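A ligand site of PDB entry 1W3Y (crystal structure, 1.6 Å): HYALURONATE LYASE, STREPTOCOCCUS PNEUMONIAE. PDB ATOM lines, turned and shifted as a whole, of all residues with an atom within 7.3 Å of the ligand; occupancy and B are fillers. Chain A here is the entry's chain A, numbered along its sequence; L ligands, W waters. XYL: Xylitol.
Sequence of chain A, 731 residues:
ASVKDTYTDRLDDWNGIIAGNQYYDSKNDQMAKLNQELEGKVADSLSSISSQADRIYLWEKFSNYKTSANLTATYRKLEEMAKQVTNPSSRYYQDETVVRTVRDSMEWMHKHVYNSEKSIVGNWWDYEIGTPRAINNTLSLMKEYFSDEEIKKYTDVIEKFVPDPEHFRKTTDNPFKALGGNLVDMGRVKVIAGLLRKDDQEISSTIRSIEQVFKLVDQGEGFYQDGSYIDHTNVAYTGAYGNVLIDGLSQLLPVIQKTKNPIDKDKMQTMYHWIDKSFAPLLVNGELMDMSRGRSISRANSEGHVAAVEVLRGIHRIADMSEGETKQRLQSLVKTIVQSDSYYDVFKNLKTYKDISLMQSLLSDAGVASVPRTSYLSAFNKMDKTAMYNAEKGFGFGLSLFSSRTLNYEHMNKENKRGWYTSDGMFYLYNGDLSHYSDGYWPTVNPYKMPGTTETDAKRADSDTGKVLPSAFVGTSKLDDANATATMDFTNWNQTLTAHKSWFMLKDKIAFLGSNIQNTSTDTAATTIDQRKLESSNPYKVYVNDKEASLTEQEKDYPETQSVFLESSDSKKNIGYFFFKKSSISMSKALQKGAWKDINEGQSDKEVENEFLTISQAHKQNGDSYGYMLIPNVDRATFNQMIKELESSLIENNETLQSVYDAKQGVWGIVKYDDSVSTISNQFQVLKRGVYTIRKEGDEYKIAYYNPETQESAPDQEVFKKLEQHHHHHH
An oxygen (O5) of the ligand lies within hydrogen-bond range of the backbone carbonyl oxygen (O) of Thr 233 (2.7 Å).
An oxygen (O1) of the ligand sits at hydrogen-bond distance from the side-chain amide oxygen (OE1) of Gln 711, 2.9 Å away.
An oxygen (O4) of the ligand lies within hydrogen-bond range of the backbone carbonyl oxygen (O) of Arg 405, 2.8 Å away.
The backbone carbonyl oxygen (O) of Lys 382 sits at hydrogen-bond distance from an oxygen (O3) of the ligand, 2.7 Å away.
Tyr 224 touches the ligand.
CB of Asn 234 touches O5 of the ligand (3.6 Å).
Thr 406 touches the ligand.
Hydrophobic or aromatic side chains within 4 Å of the ligand: Tyr 224.
Within 4 Å of the ligand: Tyr 224, Thr 233, Asn 234, Lys 382, Arg 405, Thr 406 and Gln 711.
The nearest printed residue that does not touch the ligand is Asp 218 (4.03 Å).
The backbone NH (N) of Lys 382 sits at hydrogen-bond distance from the side-chain hydroxyl (OG) of Ser 228 (3.3 Å).
The side-chain carboxylate (OD1) of Asp 384 is in salt-bridge range of the guanidinium group (NH2) of Arg 405 (2.9 Å).
The guanidinium group of Arg 405 lies close to the side-chain amide nitrogen of Gln 711 (3.4 Å).
N of Lys 382 sits at hydrogen-bond distance from OD2 of Asp 226, 2.9 Å away.
The backbone NH (N) of Ser 403 lies within hydrogen-bond range of the side-chain hydroxyl (OG1) of Thr 406, at 3.1 Å.
The side-chain carboxylate of Asp 384 sits at hydrogen-bond distance from the side-chain hydroxyl of Thr 406 (2.7 Å).
N of Thr 233 lies within hydrogen-bond range of OE2 of Glu 221.
OH of Tyr 224 sits at hydrogen-bond distance from O of Gly 220 (2.6 Å).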
ATOM      1  N   VAL A 217       6.087 -10.315   8.871  1.00  0.00           N
ATOM      2  CA  VAL A 217       5.419  -9.034   9.120  1.00  0.00           C
ATOM      3  C   VAL A 217       5.686  -8.535  10.527  1.00  0.00           C
ATOM      4  O   VAL A 217       6.086  -9.306  11.396  1.00  0.00           O
ATOM      5  CB  VAL A 217       3.884  -9.130   8.916  1.00  0.00           C
ATOM      6  CG1 VAL A 217       3.582  -9.690   7.533  1.00  0.00           C
ATOM      7  CG2 VAL A 217       3.254  -9.992   9.997  1.00  0.00           C
ATOM      8  N   ASP A 218       5.483  -7.251  10.756  1.00  0.00           N
ATOM      9  CA  ASP A 218       5.674  -6.674  12.078  1.00  0.00           C
ATOM     10  C   ASP A 218       4.398  -5.979  12.518  1.00  0.00           C
ATOM     11  O   ASP A 218       4.363  -5.321  13.547  1.00  0.00           O
ATOM     12  CB  ASP A 218       6.852  -5.693  12.068  1.00  0.00           C
ATOM     13  CG  ASP A 218       6.885  -4.847  10.825  1.00  0.00           C
ATOM     14  OD1 ASP A 218       7.822  -5.026  10.016  1.00  0.00           O
ATOM     15  OD2 ASP A 218       5.963  -4.016  10.654  1.00  0.00           O
ATOM     16  N   GLN A 219       3.353  -6.151  11.717  1.00  0.00           N
ATOM     17  CA  GLN A 219       2.058  -5.565  11.997  1.00  0.00           C
ATOM     18  C   GLN A 219       1.026  -6.240  11.091  1.00  0.00           C
ATOM     19  O   GLN A 219       1.372  -6.771  10.040  1.00  0.00           O
ATOM     20  CB  GLN A 219       2.113  -4.054  11.728  1.00  0.00           C
ATOM     21  CG  GLN A 219       0.958  -3.261  12.284  1.00  0.00           C
ATOM     22  CD  GLN A 219       1.185  -1.760  12.147  1.00  0.00           C
ATOM     23  OE1 GLN A 219       1.914  -1.148  12.933  1.00  0.00           O
ATOM     24  NE2 GLN A 219       0.576  -1.170  11.130  1.00  0.00           N
ATOM     25  N   GLY A 220      -0.239  -6.251  11.510  1.00  0.00           N
ATOM     26  CA  GLY A 220      -1.267  -6.865  10.698  1.00  0.00           C
ATOM     27  C   GLY A 220      -1.284  -8.393  10.708  1.00  0.00           C
ATOM     28  O   GLY A 220      -0.749  -9.021  11.606  1.00  0.00           O
ATOM     29  N   GLU A 221      -1.899  -8.974   9.689  1.00  0.00           N
ATOM     30  CA  GLU A 221      -2.025 -10.421   9.568  1.00  0.00           C
ATOM     31  C   GLU A 221      -0.783 -11.106   9.008  1.00  0.00           C
ATOM     32  O   GLU A 221      -0.096 -10.559   8.139  1.00  0.00           O
ATOM     33  CB  GLU A 221      -3.248 -10.759   8.702  1.00  0.00           C
ATOM     34  CG  GLU A 221      -4.494  -9.973   9.102  1.00  0.00           C
ATOM     35  CD  GLU A 221      -5.661 -10.159   8.150  1.00  0.00           C
ATOM     36  OE1 GLU A 221      -5.410 -10.394   6.946  1.00  0.00           O
ATOM     37  OE2 GLU A 221      -6.816 -10.064   8.600  1.00  0.00           O
ATOM     38  N   TYR A 224       5.043 -13.510  12.515  1.00  0.00           N
ATOM     39  CA  TYR A 224       5.953 -12.555  13.122  1.00  0.00           C
ATOM     40  C   TYR A 224       7.264 -13.259  13.478  1.00  0.00           C
ATOM     41  O   TYR A 224       7.302 -14.492  13.553  1.00  0.00           O
ATOM     42  CB  TYR A 224       5.336 -11.962  14.387  1.00  0.00           C
ATOM     43  CG  TYR A 224       4.182 -11.025  14.133  1.00  0.00           C
ATOM     44  CD1 TYR A 224       2.974 -11.484  13.606  1.00  0.00           C
ATOM     45  CD2 TYR A 224       4.300  -9.660  14.419  1.00  0.00           C
ATOM     46  CE1 TYR A 224       1.905 -10.613  13.365  1.00  0.00           C
ATOM     47  CE2 TYR A 224       3.246  -8.778  14.189  1.00  0.00           C
ATOM     48  CZ  TYR A 224       2.054  -9.263  13.659  1.00  0.00           C
ATOM     49  OH  TYR A 224       1.013  -8.382  13.441  1.00  0.00           O
ATOM     50  N   ASP A 226       8.686 -13.673  16.191  1.00  0.00           N
ATOM     51  CA  ASP A 226       8.658 -14.487  17.409  1.00  0.00           C
ATOM     52  C   ASP A 226       7.794 -15.727  17.264  1.00  0.00           C
ATOM     53  O   ASP A 226       7.561 -16.460  18.233  1.00  0.00           O
ATOM     54  CB  ASP A 226       8.205 -13.656  18.633  1.00  0.00           C
ATOM     55  CG  ASP A 226       6.740 -13.279  18.601  1.00  0.00           C
ATOM     56  OD1 ASP A 226       6.008 -13.671  17.667  1.00  0.00           O
ATOM     57  OD2 ASP A 226       6.306 -12.567  19.539  1.00  0.00           O
ATOM     58  N   SER A 228       4.556 -15.832  16.304  1.00  0.00           N
ATOM     59  CA  SER A 228       3.122 -15.556  16.364  1.00  0.00           C
ATOM     60  C   SER A 228       2.514 -15.519  14.963  1.00  0.00           C
ATOM     61  O   SER A 228       3.187 -15.194  13.993  1.00  0.00           O
ATOM     62  CB  SER A 228       2.874 -14.204  17.026  1.00  0.00           C
ATOM     63  OG  SER A 228       3.391 -14.159  18.349  1.00  0.00           O
ATOM     64  N   ILE A 230      -1.087 -14.019  13.225  1.00  0.00           N
ATOM     65  CA  ILE A 230      -2.309 -13.250  13.406  1.00  0.00           C
ATOM     66  C   ILE A 230      -3.195 -13.310  12.161  1.00  0.00           C
ATOM     67  O   ILE A 230      -2.691 -13.294  11.049  1.00  0.00           O
ATOM     68  CB  ILE A 230      -1.992 -11.745  13.650  1.00  0.00           C
ATOM     69  CG1 ILE A 230      -1.305 -11.559  15.009  1.00  0.00           C
ATOM     70  CG2 ILE A 230      -3.270 -10.911  13.556  1.00  0.00           C
ATOM     71  CD1 ILE A 230      -2.212 -11.787  16.203  1.00  0.00           C
ATOM     72  N   ASP A 231      -4.502 -13.422  12.363  1.00  0.00           N
ATOM     73  CA  ASP A 231      -5.412 -13.375  11.231  1.00  0.00           C
ATOM     74  C   ASP A 231      -6.654 -12.620  11.687  1.00  0.00           C
ATOM     75  O   ASP A 231      -6.790 -12.323  12.879  1.00  0.00           O
ATOM     76  CB  ASP A 231      -5.785 -14.775  10.726  1.00  0.00           C
ATOM     77  CG  ASP A 231      -6.018 -14.787   9.206  1.00  0.00           C
ATOM     78  OD1 ASP A 231      -6.727 -13.889   8.710  1.00  0.00           O
ATOM     79  OD2 ASP A 231      -5.480 -15.684   8.519  1.00  0.00           O
ATOM     80  N   HIS A 232      -7.540 -12.299  10.751  1.00  0.00           N
ATOM     81  CA  HIS A 232      -8.736 -11.551  11.073  1.00  0.00           C
ATOM     82  C   HIS A 232      -8.393 -10.287  11.861  1.00  0.00           C
ATOM     83  O   HIS A 232      -8.964 -10.025  12.919  1.00  0.00           O
ATOM     84  CB  HIS A 232      -9.733 -12.428  11.853  1.00  0.00           C
ATOM     85  CG  HIS A 232     -10.444 -13.415  10.985  1.00  0.00           C
ATOM     86  ND1 HIS A 232     -11.433 -14.254  11.473  1.00  0.00           N
ATOM     87  CD2 HIS A 232     -10.341 -13.682   9.660  1.00  0.00           C
ATOM     88  CE1 HIS A 232     -11.905 -14.982  10.479  1.00  0.00           C
ATOM     89  NE2 HIS A 232     -11.267 -14.663   9.371  1.00  0.00           N
ATOM     90  N   THR A 233      -7.456  -9.529  11.315  1.00  0.00           N
ATOM     91  CA  THR A 233      -6.986  -8.259  11.876  1.00  0.00           C
ATOM     92  C   THR A 233      -6.128  -8.331  13.128  1.00  0.00           C
ATOM     93  O   THR A 233      -5.007  -7.827  13.132  1.00  0.00           O
ATOM     94  CB  THR A 233      -8.176  -7.301  12.176  1.00  0.00           C
ATOM     95  OG1 THR A 233      -8.962  -7.122  11.001  1.00  0.00           O
ATOM     96  CG2 THR A 233      -7.648  -5.940  12.640  1.00  0.00           C
ATOM     97  N   ASN A 234      -6.635  -8.965  14.182  1.00  0.00           N
ATOM     98  CA  ASN A 234      -5.886  -9.028  15.435  1.00  0.00           C
ATOM     99  C   ASN A 234      -6.194 -10.237  16.323  1.00  0.00           C
ATOM    100  O   ASN A 234      -6.222 -10.106  17.548  1.00  0.00           O
ATOM    101  CB  ASN A 234      -6.139  -7.740  16.229  1.00  0.00           C
ATOM    102  CG  ASN A 234      -7.607  -7.536  16.562  1.00  0.00           C
ATOM    103  OD1 ASN A 234      -8.475  -8.280  16.092  1.00  0.00           O
ATOM    104  ND2 ASN A 234      -7.896  -6.524  17.372  1.00  0.00           N
ATOM    105  N   VAL A 235      -6.419 -11.387  15.720  1.00  0.00           N
ATOM    106  CA  VAL A 235      -6.718 -12.598  16.487  1.00  0.00           C
ATOM    107  C   VAL A 235      -5.604 -13.645  16.384  1.00  0.00           C
ATOM    108  O   VAL A 235      -5.129 -13.937  15.285  1.00  0.00           O
ATOM    109  CB  VAL A 235      -8.042 -13.256  15.994  1.00  0.00           C
ATOM    110  CG1 VAL A 235      -8.420 -14.429  16.907  1.00  0.00           C
ATOM    111  CG2 VAL A 235      -9.159 -12.226  15.936  1.00  0.00           C
ATOM    112  N   ASN A 381       4.701 -13.310  22.046  1.00  0.00           N
ATOM    113  CA  ASN A 381       4.252 -12.004  22.458  1.00  0.00           C
ATOM    114  C   ASN A 381       3.424 -11.221  21.439  1.00  0.00           C
ATOM    115  O   ASN A 381       2.541 -10.457  21.817  1.00  0.00           O
ATOM    116  CB  ASN A 381       5.451 -11.168  22.914  1.00  0.00           C
ATOM    117  CG  ASN A 381       5.901 -11.530  24.321  1.00  0.00           C
ATOM    118  OD1 ASN A 381       5.074 -11.628  25.232  1.00  0.00           O
ATOM    119  ND2 ASN A 381       7.205 -11.712  24.512  1.00  0.00           N
ATOM    120  N   LYS A 382       3.693 -11.419  20.150  1.00  0.00           N
ATOM    121  CA  LYS A 382       2.932 -10.690  19.139  1.00  0.00           C
ATOM    122  C   LYS A 382       1.480 -11.171  18.998  1.00  0.00           C
ATOM    123  O   LYS A 382       0.698 -10.575  18.260  1.00  0.00           O
ATOM    124  CB  LYS A 382       3.652 -10.739  17.784  1.00  0.00           C
ATOM    125  CG  LYS A 382       5.023 -10.051  17.809  1.00  0.00           C
ATOM    126  CD  LYS A 382       4.914  -8.592  18.240  1.00  0.00           C
ATOM    127  CE  LYS A 382       6.284  -7.934  18.382  1.00  0.00           C
ATOM    128  NZ  LYS A 382       7.055  -7.959  17.103  1.00  0.00           N
ATOM    129  N   MET A 383       1.122 -12.255  19.695  1.00  0.00           N
ATOM    130  CA  MET A 383      -0.275 -12.705  19.690  1.00  0.00           C
ATOM    131  C   MET A 383      -0.746 -12.989  21.126  1.00  0.00           C
ATOM    132  O   MET A 383      -1.804 -13.566  21.348  1.00  0.00           O
ATOM    133  CB  MET A 383      -0.495 -13.928  18.782  1.00  0.00           C
ATOM    134  CG  MET A 383       0.186 -15.221  19.172  1.00  0.00           C
ATOM    135  SD  MET A 383      -0.329 -16.530  18.026  1.00  0.00           S
ATOM    136  CE  MET A 383       0.363 -18.007  18.846  1.00  0.00           C
ATOM    137  N   ASP A 384       0.070 -12.544  22.085  1.00  0.00           N
ATOM    138  CA  ASP A 384      -0.209 -12.680  23.527  1.00  0.00           C
ATOM    139  C   ASP A 384      -0.534 -14.079  24.063  1.00  0.00           C
ATOM    140  O   ASP A 384      -1.442 -14.245  24.889  1.00  0.00           O
ATOM    141  CB  ASP A 384      -1.330 -11.693  23.925  1.00  0.00           C
ATOM    142  CG  ASP A 384      -0.950 -10.241  23.665  1.00  0.00           C
ATOM    143  OD1 ASP A 384       0.097  -9.804  24.191  1.00  0.00           O
ATOM    144  OD2 ASP A 384      -1.684  -9.530  22.948  1.00  0.00           O
ATOM    145  N   SER A 403      -4.575  -8.296  24.752  1.00  0.00           N
ATOM    146  CA  SER A 403      -4.176  -6.970  25.181  1.00  0.00           C
ATOM    147  C   SER A 403      -4.798  -5.937  24.267  1.00  0.00           C
ATOM    148  O   SER A 403      -5.722  -6.240  23.515  1.00  0.00           O
ATOM    149  CB  SER A 403      -2.645  -6.854  25.094  1.00  0.00           C
ATOM    150  OG  SER A 403      -2.228  -6.902  23.733  1.00  0.00           O
ATOM    151  N   SER A 404      -4.290  -4.714  24.309  1.00  0.00           N
ATOM    152  CA  SER A 404      -4.806  -3.668  23.440  1.00  0.00           C
ATOM    153  C   SER A 404      -4.493  -4.021  21.988  1.00  0.00           C
ATOM    154  O   SER A 404      -5.099  -3.466  21.059  1.00  0.00           O
ATOM    155  CB  SER A 404      -4.164  -2.313  23.800  1.00  0.00           C
ATOM    156  OG  SER A 404      -2.756  -2.359  23.679  1.00  0.00           O
ATOM    157  N   ARG A 405      -3.582  -4.972  21.797  1.00  0.00           N
ATOM    158  CA  ARG A 405      -3.150  -5.381  20.464  1.00  0.00           C
ATOM    159  C   ARG A 405      -3.893  -6.580  19.870  1.00  0.00           C
ATOM    160  O   ARG A 405      -3.787  -6.847  18.678  1.00  0.00           O
ATOM    161  CB  ARG A 405      -1.656  -5.729  20.495  1.00  0.00           C
ATOM    162  CG  ARG A 405      -0.730  -4.638  21.043  1.00  0.00           C
ATOM    163  CD  ARG A 405       0.694  -5.161  21.245  1.00  0.00           C
ATOM    164  NE  ARG A 405       0.755  -6.203  22.287  1.00  0.00           N
ATOM    165  CZ  ARG A 405       0.950  -5.984  23.584  1.00  0.00           C
ATOM    166  NH1 ARG A 405       1.144  -4.747  24.036  1.00  0.00           N
ATOM    167  NH2 ARG A 405       0.936  -6.997  24.436  1.00  0.00           N
ATOM    168  N   THR A 406      -4.647  -7.304  20.705  1.00  0.00           N
ATOM    169  CA  THR A 406      -5.343  -8.499  20.250  1.00  0.00           C
ATOM    170  C   THR A 406      -6.766  -8.668  20.782  1.00  0.00           C
ATOM    171  O   THR A 406      -7.080  -8.236  21.884  1.00  0.00           O
ATOM    172  CB  THR A 406      -4.544  -9.757  20.653  1.00  0.00           C
ATOM    173  OG1 THR A 406      -4.279  -9.708  22.059  1.00  0.00           O
ATOM    174  CG2 THR A 406      -3.211  -9.825  19.899  1.00  0.00           C
ATOM    175  N   LEU A 407      -7.614  -9.335  20.006  1.00  0.00           N
ATOM    176  CA  LEU A 407      -8.992  -9.584  20.393  1.00  0.00           C
ATOM    177  C   LEU A 407      -9.042 -10.748  21.386  1.00  0.00           C
ATOM    178  O   LEU A 407      -8.315 -11.743  21.204  1.00  0.00           O
ATOM    179  CB  LEU A 407      -9.825  -9.930  19.160  1.00  0.00           C
ATOM    180  CG  LEU A 407     -11.328  -9.658  19.221  1.00  0.00           C
ATOM    181  CD1 LEU A 407     -11.572  -8.157  19.184  1.00  0.00           C
ATOM    182  CD2 LEU A 407     -12.018 -10.331  18.051  1.00  0.00           C
ATOM    183  N   TYR A 706      11.655  -7.617  29.708  1.00  0.00           N
ATOM    184  CA  TYR A 706      10.730  -7.293  28.632  1.00  0.00           C
ATOM    185  C   TYR A 706       9.734  -6.225  29.068  1.00  0.00           C
ATOM    186  O   TYR A 706       9.102  -6.332  30.112  1.00  0.00           O
ATOM    187  CB  TYR A 706       9.972  -8.539  28.166  1.00  0.00           C
ATOM    188  CG  TYR A 706       9.052  -8.311  26.973  1.00  0.00           C
ATOM    189  CD1 TYR A 706       9.557  -7.834  25.769  1.00  0.00           C
ATOM    190  CD2 TYR A 706       7.677  -8.572  27.065  1.00  0.00           C
ATOM    191  CE1 TYR A 706       8.726  -7.628  24.665  1.00  0.00           C
ATOM    192  CE2 TYR A 706       6.838  -8.371  25.961  1.00  0.00           C
ATOM    193  CZ  TYR A 706       7.369  -7.900  24.762  1.00  0.00           C
ATOM    194  OH  TYR A 706       6.548  -7.711  23.662  1.00  0.00           O
ATOM    195  N   GLN A 711       7.018  -3.220  23.751  1.00  0.00           N
ATOM    196  CA  GLN A 711       7.428  -4.450  23.065  1.00  0.00           C
ATOM    197  C   GLN A 711       8.930  -4.423  22.783  1.00  0.00           C
ATOM    198  O   GLN A 711       9.383  -4.674  21.664  1.00  0.00           O
ATOM    199  CB  GLN A 711       6.656  -4.616  21.752  1.00  0.00           C
ATOM    200  CG  GLN A 711       5.162  -4.825  21.951  1.00  0.00           C
ATOM    201  CD  GLN A 711       4.457  -5.248  20.678  1.00  0.00           C
ATOM    202  OE1 GLN A 711       4.535  -4.559  19.651  1.00  0.00           O
ATOM    203  NE2 GLN A 711       3.762  -6.379  20.725  1.00  0.00           N
HETATM  204  C1  XYL L   1       2.197  -6.375  16.773  1.00  0.00           C
HETATM  205  C2  XYL L   1       1.054  -6.652  17.744  1.00  0.00           C
HETATM  206  C3  XYL L   1      -0.045  -7.513  17.052  1.00  0.00           C
HETATM  207  C4  XYL L   1      -1.029  -6.664  16.233  1.00  0.00           C
HETATM  208  C5  XYL L   1      -1.950  -7.447  15.300  1.00  0.00           C
HETATM  209  O1  XYL L   1       2.913  -5.264  17.316  1.00  0.00           O
HETATM  210  O2  XYL L   1       1.578  -7.401  18.844  1.00  0.00           O
HETATM  211  O3  XYL L   1      -0.756  -8.358  17.964  1.00  0.00           O
HETATM  212  O4  XYL L   1      -1.848  -5.797  17.025  1.00  0.00           O
HETATM  213  O5  XYL L   1      -3.073  -6.745  14.739  1.00  0.00           O
HETATM  214  O   HOH W   1       0.405  -8.792  21.111  1.00  0.00           O
HETATM  215  O   HOH W   2       1.723  -2.925  18.148  1.00  0.00           O
